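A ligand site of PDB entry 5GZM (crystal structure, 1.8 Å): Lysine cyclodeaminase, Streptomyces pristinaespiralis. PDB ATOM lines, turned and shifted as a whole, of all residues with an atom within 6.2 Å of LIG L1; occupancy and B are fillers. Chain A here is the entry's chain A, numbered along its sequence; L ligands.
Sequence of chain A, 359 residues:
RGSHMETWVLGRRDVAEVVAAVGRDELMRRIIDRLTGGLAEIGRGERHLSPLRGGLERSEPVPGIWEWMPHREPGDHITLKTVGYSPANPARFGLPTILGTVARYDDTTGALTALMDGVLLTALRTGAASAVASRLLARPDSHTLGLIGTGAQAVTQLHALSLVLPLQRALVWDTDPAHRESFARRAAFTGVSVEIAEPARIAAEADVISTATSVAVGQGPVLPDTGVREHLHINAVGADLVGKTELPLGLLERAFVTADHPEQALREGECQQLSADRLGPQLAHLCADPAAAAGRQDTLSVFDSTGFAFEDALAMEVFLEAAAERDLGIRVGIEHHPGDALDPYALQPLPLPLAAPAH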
ATOM      1  N   ARG A  53     -19.449 -18.496   6.440  1.00  0.00           N
ATOM      2  CA  ARG A  53     -20.325 -19.606   6.616  1.00  0.00           C
ATOM      3  C   ARG A  53     -20.973 -19.368   7.924  1.00  0.00           C
ATOM      4  O   ARG A  53     -20.594 -18.449   8.657  1.00  0.00           O
ATOM      5  CB  ARG A  53     -19.512 -20.886   6.669  1.00  0.00           C
ATOM      6  CG  ARG A  53     -18.440 -20.942   7.745  1.00  0.00           C
ATOM      7  CD  ARG A  53     -17.542 -22.134   7.433  1.00  0.00           C
ATOM      8  NE  ARG A  53     -16.292 -22.066   8.176  1.00  0.00           N
ATOM      9  CZ  ARG A  53     -15.260 -22.885   7.991  1.00  0.00           C
ATOM     10  NH1 ARG A  53     -15.315 -23.885   7.104  1.00  0.00           N
ATOM     11  NH2 ARG A  53     -14.173 -22.704   8.664  1.00  0.00           N
ATOM     12  N   ILE A  65     -19.488 -27.748  16.711  1.00  0.00           N
ATOM     13  CA  ILE A  65     -20.131 -26.773  15.840  1.00  0.00           C
ATOM     14  C   ILE A  65     -20.791 -27.534  14.640  1.00  0.00           C
ATOM     15  O   ILE A  65     -20.286 -28.542  14.173  1.00  0.00           O
ATOM     16  CB  ILE A  65     -19.196 -25.607  15.453  1.00  0.00           C
ATOM     17  CG1 ILE A  65     -19.984 -24.442  14.835  1.00  0.00           C
ATOM     18  CG2 ILE A  65     -18.053 -25.995  14.534  1.00  0.00           C
ATOM     19  CD1 ILE A  65     -19.415 -23.046  15.075  1.00  0.00           C
ATOM     20  N   GLU A  67     -22.160 -26.432  10.869  1.00  0.00           N
ATOM     21  CA  GLU A  67     -22.062 -25.306   9.963  1.00  0.00           C
ATOM     22  C   GLU A  67     -22.725 -25.539   8.613  1.00  0.00           C
ATOM     23  O   GLU A  67     -22.774 -26.684   8.147  1.00  0.00           O
ATOM     24  CB  GLU A  67     -20.592 -24.994   9.752  1.00  0.00           C
ATOM     25  CG  GLU A  67     -19.952 -24.270  10.951  1.00  0.00           C
ATOM     26  CD  GLU A  67     -18.440 -24.307  10.886  1.00  0.00           C
ATOM     27  OE1 GLU A  67     -17.866 -24.553   9.802  1.00  0.00           O
ATOM     28  OE2 GLU A  67     -17.824 -24.135  11.947  1.00  0.00           O
ATOM     29  N   MET A  69     -22.255 -24.033   4.611  1.00  0.00           N
ATOM     30  CA  MET A  69     -21.231 -23.320   3.861  1.00  0.00           C
ATOM     31  C   MET A  69     -21.719 -23.186   2.421  1.00  0.00           C
ATOM     32  O   MET A  69     -21.622 -24.158   1.650  1.00  0.00           O
ATOM     33  CB  MET A  69     -19.955 -24.171   3.849  1.00  0.00           C
ATOM     34  CG  MET A  69     -19.420 -24.481   5.259  1.00  0.00           C
ATOM     35  SD  MET A  69     -18.040 -25.655   5.326  1.00  0.00           S
ATOM     36  CE  MET A  69     -16.919 -24.882   4.106  1.00  0.00           C
ATOM     37  N   LYS A  81     -22.564 -27.060   1.517  1.00  0.00           N
ATOM     38  CA  LYS A  81     -22.136 -28.106   2.415  1.00  0.00           C
ATOM     39  C   LYS A  81     -22.655 -27.891   3.794  1.00  0.00           C
ATOM     40  O   LYS A  81     -22.588 -26.759   4.355  1.00  0.00           O
ATOM     41  CB  LYS A  81     -20.599 -28.224   2.456  1.00  0.00           C
ATOM     42  CG  LYS A  81     -20.173 -29.481   3.238  1.00  0.00           C
ATOM     43  CD  LYS A  81     -18.733 -29.923   2.994  1.00  0.00           C
ATOM     44  CE  LYS A  81     -17.777 -29.092   3.850  1.00  0.00           C
ATOM     45  NZ  LYS A  81     -16.337 -29.497   3.728  1.00  0.00           N
ATOM     46  N   VAL A  83     -22.114 -29.536   7.541  1.00  0.00           N
ATOM     47  CA  VAL A  83     -21.075 -30.267   8.188  1.00  0.00           C
ATOM     48  C   VAL A  83     -20.967 -29.983   9.692  1.00  0.00           C
ATOM     49  O   VAL A  83     -21.063 -28.806  10.111  1.00  0.00           O
ATOM     50  CB  VAL A  83     -19.753 -29.971   7.474  1.00  0.00           C
ATOM     51  CG1 VAL A  83     -19.348 -28.516   7.628  1.00  0.00           C
ATOM     52  CG2 VAL A  83     -18.661 -30.933   7.957  1.00  0.00           C
ATOM     53  N   GLY A  84     -20.839 -31.072  10.461  1.00  0.00           N
ATOM     54  CA  GLY A  84     -20.642 -31.074  11.880  1.00  0.00           C
ATOM     55  C   GLY A  84     -19.207 -31.371  12.196  1.00  0.00           C
ATOM     56  O   GLY A  84     -18.544 -32.111  11.468  1.00  0.00           O
ATOM     57  N   TYR A  85     -18.737 -30.663  13.213  1.00  0.00           N
ATOM     58  CA  TYR A  85     -17.543 -31.006  13.953  1.00  0.00           C
ATOM     59  C   TYR A  85     -18.015 -31.419  15.343  1.00  0.00           C
ATOM     60  O   TYR A  85     -18.461 -30.557  16.150  1.00  0.00           O
ATOM     61  CB  TYR A  85     -16.686 -29.801  14.102  1.00  0.00           C
ATOM     62  CG  TYR A  85     -15.562 -29.938  15.078  1.00  0.00           C
ATOM     63  CD1 TYR A  85     -14.481 -30.781  14.821  1.00  0.00           C
ATOM     64  CD2 TYR A  85     -15.534 -29.173  16.209  1.00  0.00           C
ATOM     65  CE1 TYR A  85     -13.436 -30.873  15.723  1.00  0.00           C
ATOM     66  CE2 TYR A  85     -14.489 -29.265  17.111  1.00  0.00           C
ATOM     67  CZ  TYR A  85     -13.446 -30.119  16.845  1.00  0.00           C
ATOM     68  OH  TYR A  85     -12.411 -30.159  17.752  1.00  0.00           O
ATOM     69  N   ILE A  98     -15.907 -35.316  11.606  1.00  0.00           N
ATOM     70  CA  ILE A  98     -16.423 -34.449  10.519  1.00  0.00           C
ATOM     71  C   ILE A  98     -17.438 -35.291   9.743  1.00  0.00           C
ATOM     72  O   ILE A  98     -17.072 -36.268   9.112  1.00  0.00           O
ATOM     73  CB  ILE A  98     -15.301 -33.943   9.616  1.00  0.00           C
ATOM     74  CG1 ILE A  98     -14.334 -33.044  10.415  1.00  0.00           C
ATOM     75  CG2 ILE A  98     -15.864 -33.160   8.436  1.00  0.00           C
ATOM     76  CD1 ILE A  98     -14.962 -31.789  11.000  1.00  0.00           C
ATOM     77  N   THR A 122     -14.542 -33.870   1.703  1.00  0.00           N
ATOM     78  CA  THR A 122     -13.901 -32.898   2.649  1.00  0.00           C
ATOM     79  C   THR A 122     -12.448 -33.259   2.882  1.00  0.00           C
ATOM     80  O   THR A 122     -11.528 -32.444   2.667  1.00  0.00           O
ATOM     81  CB  THR A 122     -14.639 -32.765   3.981  1.00  0.00           C
ATOM     82  OG1 THR A 122     -15.962 -32.298   3.744  1.00  0.00           O
ATOM     83  CG2 THR A 122     -13.954 -31.742   4.882  1.00  0.00           C
ATOM     84  N   ARG A 125     -10.423 -32.549  -0.505  1.00  0.00           N
ATOM     85  CA  ARG A 125     -10.114 -31.146  -0.856  1.00  0.00           C
ATOM     86  C   ARG A 125      -9.249 -30.450   0.213  1.00  0.00           C
ATOM     87  O   ARG A 125      -8.502 -29.514  -0.135  1.00  0.00           O
ATOM     88  CB  ARG A 125     -11.336 -30.286  -1.268  1.00  0.00           C
ATOM     89  CG  ARG A 125     -12.440 -30.082  -0.270  1.00  0.00           C
ATOM     90  CD  ARG A 125     -12.047 -29.210   0.942  1.00  0.00           C
ATOM     91  NE  ARG A 125     -13.162 -28.497   1.523  1.00  0.00           N
ATOM     92  CZ  ARG A 125     -13.167 -27.934   2.737  1.00  0.00           C
ATOM     93  NH1 ARG A 125     -14.191 -27.223   3.131  1.00  0.00           N
ATOM     94  NH2 ARG A 125     -12.164 -28.097   3.546  1.00  0.00           N
ATOM     95  N   THR A 126      -9.220 -30.964   1.423  1.00  0.00           N
ATOM     96  CA  THR A 126      -8.440 -30.335   2.490  1.00  0.00           C
ATOM     97  C   THR A 126      -7.004 -30.786   2.343  1.00  0.00           C
ATOM     98  O   THR A 126      -6.053 -29.958   2.455  1.00  0.00           O
ATOM     99  CB  THR A 126      -9.011 -30.742   3.865  1.00  0.00           C
ATOM    100  OG1 THR A 126     -10.400 -30.330   3.927  1.00  0.00           O
ATOM    101  CG2 THR A 126      -8.258 -30.093   5.003  1.00  0.00           C
ATOM    102  N   ALA A 239      -9.358 -26.488  13.008  1.00  0.00           N
ATOM    103  CA  ALA A 239     -10.242 -25.296  13.116  1.00  0.00           C
ATOM    104  C   ALA A 239     -11.736 -25.630  13.166  1.00  0.00           C
ATOM    105  O   ALA A 239     -12.264 -26.380  12.404  1.00  0.00           O
ATOM    106  CB  ALA A 239      -9.991 -24.249  12.101  1.00  0.00           C
ATOM    107  N   ASP A 240     -12.375 -24.949  14.064  1.00  0.00           N
ATOM    108  CA  ASP A 240     -13.752 -25.210  14.393  1.00  0.00           C
ATOM    109  C   ASP A 240     -14.222 -24.007  15.187  1.00  0.00           C
ATOM    110  O   ASP A 240     -14.711 -23.037  14.638  1.00  0.00           O
ATOM    111  CB  ASP A 240     -13.833 -26.542  15.175  1.00  0.00           C
ATOM    112  CG  ASP A 240     -12.541 -26.844  15.999  1.00  0.00           C
ATOM    113  OD1 ASP A 240     -12.383 -26.195  17.064  1.00  0.00           O
ATOM    114  OD2 ASP A 240     -11.718 -27.696  15.585  1.00  0.00           O
ATOM    115  N   GLU A 268     -11.459 -17.411  12.992  1.00  0.00           N
ATOM    116  CA  GLU A 268     -11.479 -18.805  13.480  1.00  0.00           C
ATOM    117  C   GLU A 268     -10.288 -19.678  13.075  1.00  0.00           C
ATOM    118  O   GLU A 268     -10.222 -20.850  13.464  1.00  0.00           O
ATOM    119  CB  GLU A 268     -12.751 -19.538  13.045  1.00  0.00           C
ATOM    120  CG  GLU A 268     -12.909 -19.587  11.540  1.00  0.00           C
ATOM    121  CD  GLU A 268     -14.221 -20.185  11.091  1.00  0.00           C
ATOM    122  OE1 GLU A 268     -15.284 -19.702  11.479  1.00  0.00           O
ATOM    123  OE2 GLU A 268     -14.171 -21.164  10.307  1.00  0.00           O
ATOM    124  N   THR A 306      -8.740 -23.050   6.750  1.00  0.00           N
ATOM    125  CA  THR A 306     -10.016 -23.106   7.469  1.00  0.00           C
ATOM    126  C   THR A 306     -11.132 -23.872   6.721  1.00  0.00           C
ATOM    127  O   THR A 306     -12.049 -24.341   7.346  1.00  0.00           O
ATOM    128  CB  THR A 306     -10.540 -21.691   7.842  1.00  0.00           C
ATOM    129  OG1 THR A 306     -10.754 -20.879   6.666  1.00  0.00           O
ATOM    130  CG2 THR A 306      -9.487 -20.986   8.736  1.00  0.00           C
ATOM    131  N   GLY A 307     -11.053 -23.885   5.408  1.00  0.00           N
ATOM    132  CA  GLY A 307     -11.999 -24.601   4.533  1.00  0.00           C
ATOM    133  C   GLY A 307     -13.074 -23.649   4.086  1.00  0.00           C
ATOM    134  O   GLY A 307     -13.664 -22.912   4.903  1.00  0.00           O
ATOM    135  N   PHE A 308     -13.396 -23.641   2.785  1.00  0.00           N
ATOM    136  CA  PHE A 308     -14.486 -22.849   2.302  1.00  0.00           C
ATOM    137  C   PHE A 308     -15.182 -23.512   1.153  1.00  0.00           C
ATOM    138  O   PHE A 308     -14.611 -24.348   0.469  1.00  0.00           O
ATOM    139  CB  PHE A 308     -14.094 -21.370   1.974  1.00  0.00           C
ATOM    140  CG  PHE A 308     -13.038 -21.208   0.901  1.00  0.00           C
ATOM    141  CD1 PHE A 308     -11.695 -21.526   1.140  1.00  0.00           C
ATOM    142  CD2 PHE A 308     -13.392 -20.705  -0.323  1.00  0.00           C
ATOM    143  CE1 PHE A 308     -10.730 -21.376   0.167  1.00  0.00           C
ATOM    144  CE2 PHE A 308     -12.421 -20.516  -1.320  1.00  0.00           C
ATOM    145  CZ  PHE A 308     -11.070 -20.847  -1.055  1.00  0.00           C
ATOM    146  N   GLU A 311     -14.126 -24.710  -2.410  1.00  0.00           N
ATOM    147  CA  GLU A 311     -13.295 -25.923  -2.472  1.00  0.00           C
ATOM    148  C   GLU A 311     -14.167 -27.161  -2.599  1.00  0.00           C
ATOM    149  O   GLU A 311     -13.871 -28.088  -3.353  1.00  0.00           O
ATOM    150  CB  GLU A 311     -12.387 -26.048  -1.280  1.00  0.00           C
ATOM    151  CG  GLU A 311     -11.517 -24.830  -1.017  1.00  0.00           C
ATOM    152  CD  GLU A 311     -10.621 -24.997   0.177  1.00  0.00           C
ATOM    153  OE1 GLU A 311     -11.074 -25.583   1.193  1.00  0.00           O
ATOM    154  OE2 GLU A 311      -9.448 -24.476   0.142  1.00  0.00           O
ATOM    155  N   ASP A 312     -15.266 -27.167  -1.862  1.00  0.00           N
ATOM    156  CA  ASP A 312     -16.222 -28.275  -1.890  1.00  0.00           C
ATOM    157  C   ASP A 312     -16.891 -28.353  -3.253  1.00  0.00           C
ATOM    158  O   ASP A 312     -17.091 -29.448  -3.755  1.00  0.00           O
ATOM    159  CB  ASP A 312     -17.239 -28.163  -0.743  1.00  0.00           C
ATOM    160  CG  ASP A 312     -16.548 -28.138   0.612  1.00  0.00           C
ATOM    161  OD1 ASP A 312     -15.829 -29.143   0.907  1.00  0.00           O
ATOM    162  OD2 ASP A 312     -16.597 -27.093   1.328  1.00  0.00           O
HETATM  163  C1  LIG L   1     -14.624 -27.620   6.499  1.00  0.00           C
HETATM  164  N1  LIG L   1     -13.834 -26.415   8.434  1.00  0.00           N
HETATM  165  O1  LIG L   1     -15.212 -28.563   5.974  1.00  0.00           O
HETATM  166  C2  LIG L   1     -14.386 -27.720   8.054  1.00  0.00           C
HETATM  167  C3  LIG L   1     -15.704 -28.175   8.685  1.00  0.00           C
HETATM  168  C4  LIG L   1     -15.160 -26.657  10.678  1.00  0.00           C
HETATM  169  C5  LIG L   1     -13.967 -26.121   9.888  1.00  0.00           C
HETATM  170  C6  LIG L   1     -15.551 -28.077  10.211  1.00  0.00           C
HETATM  171  O2  LIG L   1     -14.308 -26.580   5.884  1.00  0.00           O
HETATM  172  P1  LG2 L   2     -10.369 -36.550  14.063  1.00  0.00           P
HETATM  173  O1  LG2 L   2     -11.206 -36.425  15.292  1.00  0.00           O
HETATM  174  O2  LG2 L   2     -10.385 -37.538  12.956  1.00  0.00           O
HETATM  175  O3  LG2 L   2      -8.805 -36.379  14.395  1.00  0.00           O
HETATM  176  C1  LG2 L   2      -8.363 -35.404  15.334  1.00  0.00           C
HETATM  177  C2  LG2 L   2      -7.192 -36.018  16.123  1.00  0.00           C
HETATM  178  O4  LG2 L   2      -6.637 -35.035  16.960  1.00  0.00           O
HETATM  179  C3  LG2 L   2      -7.703 -37.101  17.110  1.00  0.00           C
HETATM  180  O5  LG2 L   2      -7.092 -38.348  16.779  1.00  0.00           O
HETATM  181  C4  LG2 L   2      -7.336 -36.583  18.484  1.00  0.00           C
HETATM  182  O6  LG2 L   2      -6.930 -37.555  19.455  1.00  0.00           O
HETATM  183  C5  LG2 L   2      -6.166 -35.697  18.150  1.00  0.00           C
HETATM  184  N1  LG2 L   2      -5.795 -34.637  19.115  1.00  0.00           N
HETATM  185  C6  LG2 L   2      -6.579 -33.924  19.937  1.00  0.00           C
HETATM  186  N2  LG2 L   2      -5.886 -33.018  20.609  1.00  0.00           N
HETATM  187  C7  LG2 L   2      -4.589 -33.218  20.233  1.00  0.00           C
HETATM  188  C8  LG2 L   2      -3.339 -32.607  20.580  1.00  0.00           C
HETATM  189  N3  LG2 L   2      -3.373 -31.625  21.488  1.00  0.00           N
HETATM  190  N4  LG2 L   2      -2.250 -33.072  19.952  1.00  0.00           N
HETATM  191  C9  LG2 L   2      -2.286 -34.089  19.051  1.00  0.00           C
HETATM  192  N5  LG2 L   2      -3.407 -34.720  18.685  1.00  0.00           N
HETATM  193  C10 LG2 L   2      -4.539 -34.286  19.252  1.00  0.00           C
HETATM  194  O7  LG2 L   2     -10.694 -35.097  13.264  1.00  0.00           O
HETATM  195  P2  LG2 L   2     -10.253 -34.673  11.811  1.00  0.00           P
HETATM  196  O8  LG2 L   2     -11.384 -34.997  10.817  1.00  0.00           O
HETATM  197  O9  LG2 L   2      -8.884 -35.201  11.438  1.00  0.00           O
HETATM  198  O10 LG2 L   2     -10.281 -33.113  11.898  1.00  0.00           O
HETATM  199  C11 LG2 L   2      -9.203 -32.396  12.545  1.00  0.00           C
HETATM  200  C12 LG2 L   2      -9.434 -30.912  12.647  1.00  0.00           C
HETATM  201  O11 LG2 L   2      -9.371 -30.378  11.313  1.00  0.00           O
HETATM  202  C13 LG2 L   2     -10.744 -30.441  13.268  1.00  0.00           C
HETATM  203  O12 LG2 L   2     -10.468 -29.308  14.078  1.00  0.00           O
HETATM  204  C14 LG2 L   2     -11.600 -30.141  12.032  1.00  0.00           C
HETATM  205  O13 LG2 L   2     -12.651 -29.202  12.285  1.00  0.00           O
HETATM  206  C15 LG2 L   2     -10.569 -29.609  11.091  1.00  0.00           C
HETATM  207  N6  LG2 L   2     -10.859 -29.614   9.653  1.00  0.00           N
HETATM  208  C16 LG2 L   2     -10.426 -28.570   8.953  1.00  0.00           C
HETATM  209  C17 LG2 L   2     -10.657 -28.473   7.601  1.00  0.00           C
HETATM  210  C18 LG2 L   2     -10.067 -27.303   6.858  1.00  0.00           C
HETATM  211  O14 LG2 L   2      -9.149 -26.575   7.337  1.00  0.00           O
HETATM  212  N7  LG2 L   2     -10.427 -27.236   5.620  1.00  0.00           N
HETATM  213  C19 LG2 L   2     -11.319 -29.524   6.956  1.00  0.00           C
HETATM  214  C20 LG2 L   2     -11.744 -30.630   7.704  1.00  0.00           C
HETATM  215  C21 LG2 L   2     -11.488 -30.652   9.031  1.00  0.00           C
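Merely in contact with LIG L1: Glu 67, Met 69, Val 83, Ile 98, Thr 122, Ala 239 and Gly 307.
Hydrophobic or aromatic side chains that line LIG L1: Met 69, Val 83 and Ile 98.
11 residues have an atom within 4 Å of LIG L1: Arg 53, Glu 67, Met 69, Lys 81, Val 83, Ile 98, Thr 122, Arg 125, Ala 239, Thr 306 and Gly 307.
OE1 of Glu 67 is in salt-bridge range of NE of Arg 53 (3.4 Å).
NZ of Lys 81 is in hydrogen-bond range of OG1 of Thr 122 (2.8 Å).
NH1 of Arg 53 lies close to SD of Met 69, 3.7 Å away.
The guanidinium group (NH2) of Arg 53 lies within hydrogen-bond range of the backbone carbonyl oxygen (O) of Thr 306 (3.0 Å).
NH1 of Arg 53 is in hydrogen-bond range of O of Gly 307, 2.9 Å away.
NE of Arg 53 is in salt-bridge range of OE2 of Glu 268 (3.1 Å).
N of Glu 67 is in hydrogen-bond range of O of Val 83 (2.7 Å).
NE of Arg 125 is in salt-bridge range of OE1 of Glu 311 (3.6 Å).
The backbone carbonyl oxygen (O) of Ala 239 sits at hydrogen-bond distance from an oxygen (O13) of LG2 L2, 2.9 Å away.
N of Ala 239 is in hydrogen-bond range of O12 of LG2 L2 (3.2 Å).
The guanidinium group (NH1) of Arg 125 lies within salt-bridge range of an oxygen (O2) of LIG L1 (2.8 Å).
NH1 of Arg 53 lies within salt-bridge range of O2 of LIG L1 (3.1 Å).
The backbone carbonyl oxygen (O) of Thr 306 lies within hydrogen-bond range of a nitrogen (N1) of LIG L1 (2.9 Å).
The side-chain amino group (NZ) of Lys 81 lies within salt-bridge range of an oxygen (O1) of LIG L1.
The side-chain carboxylate (OD2) of Asp 240 sits at hydrogen-bond distance from an oxygen (O12) of LG2 L2 (2.5 Å).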
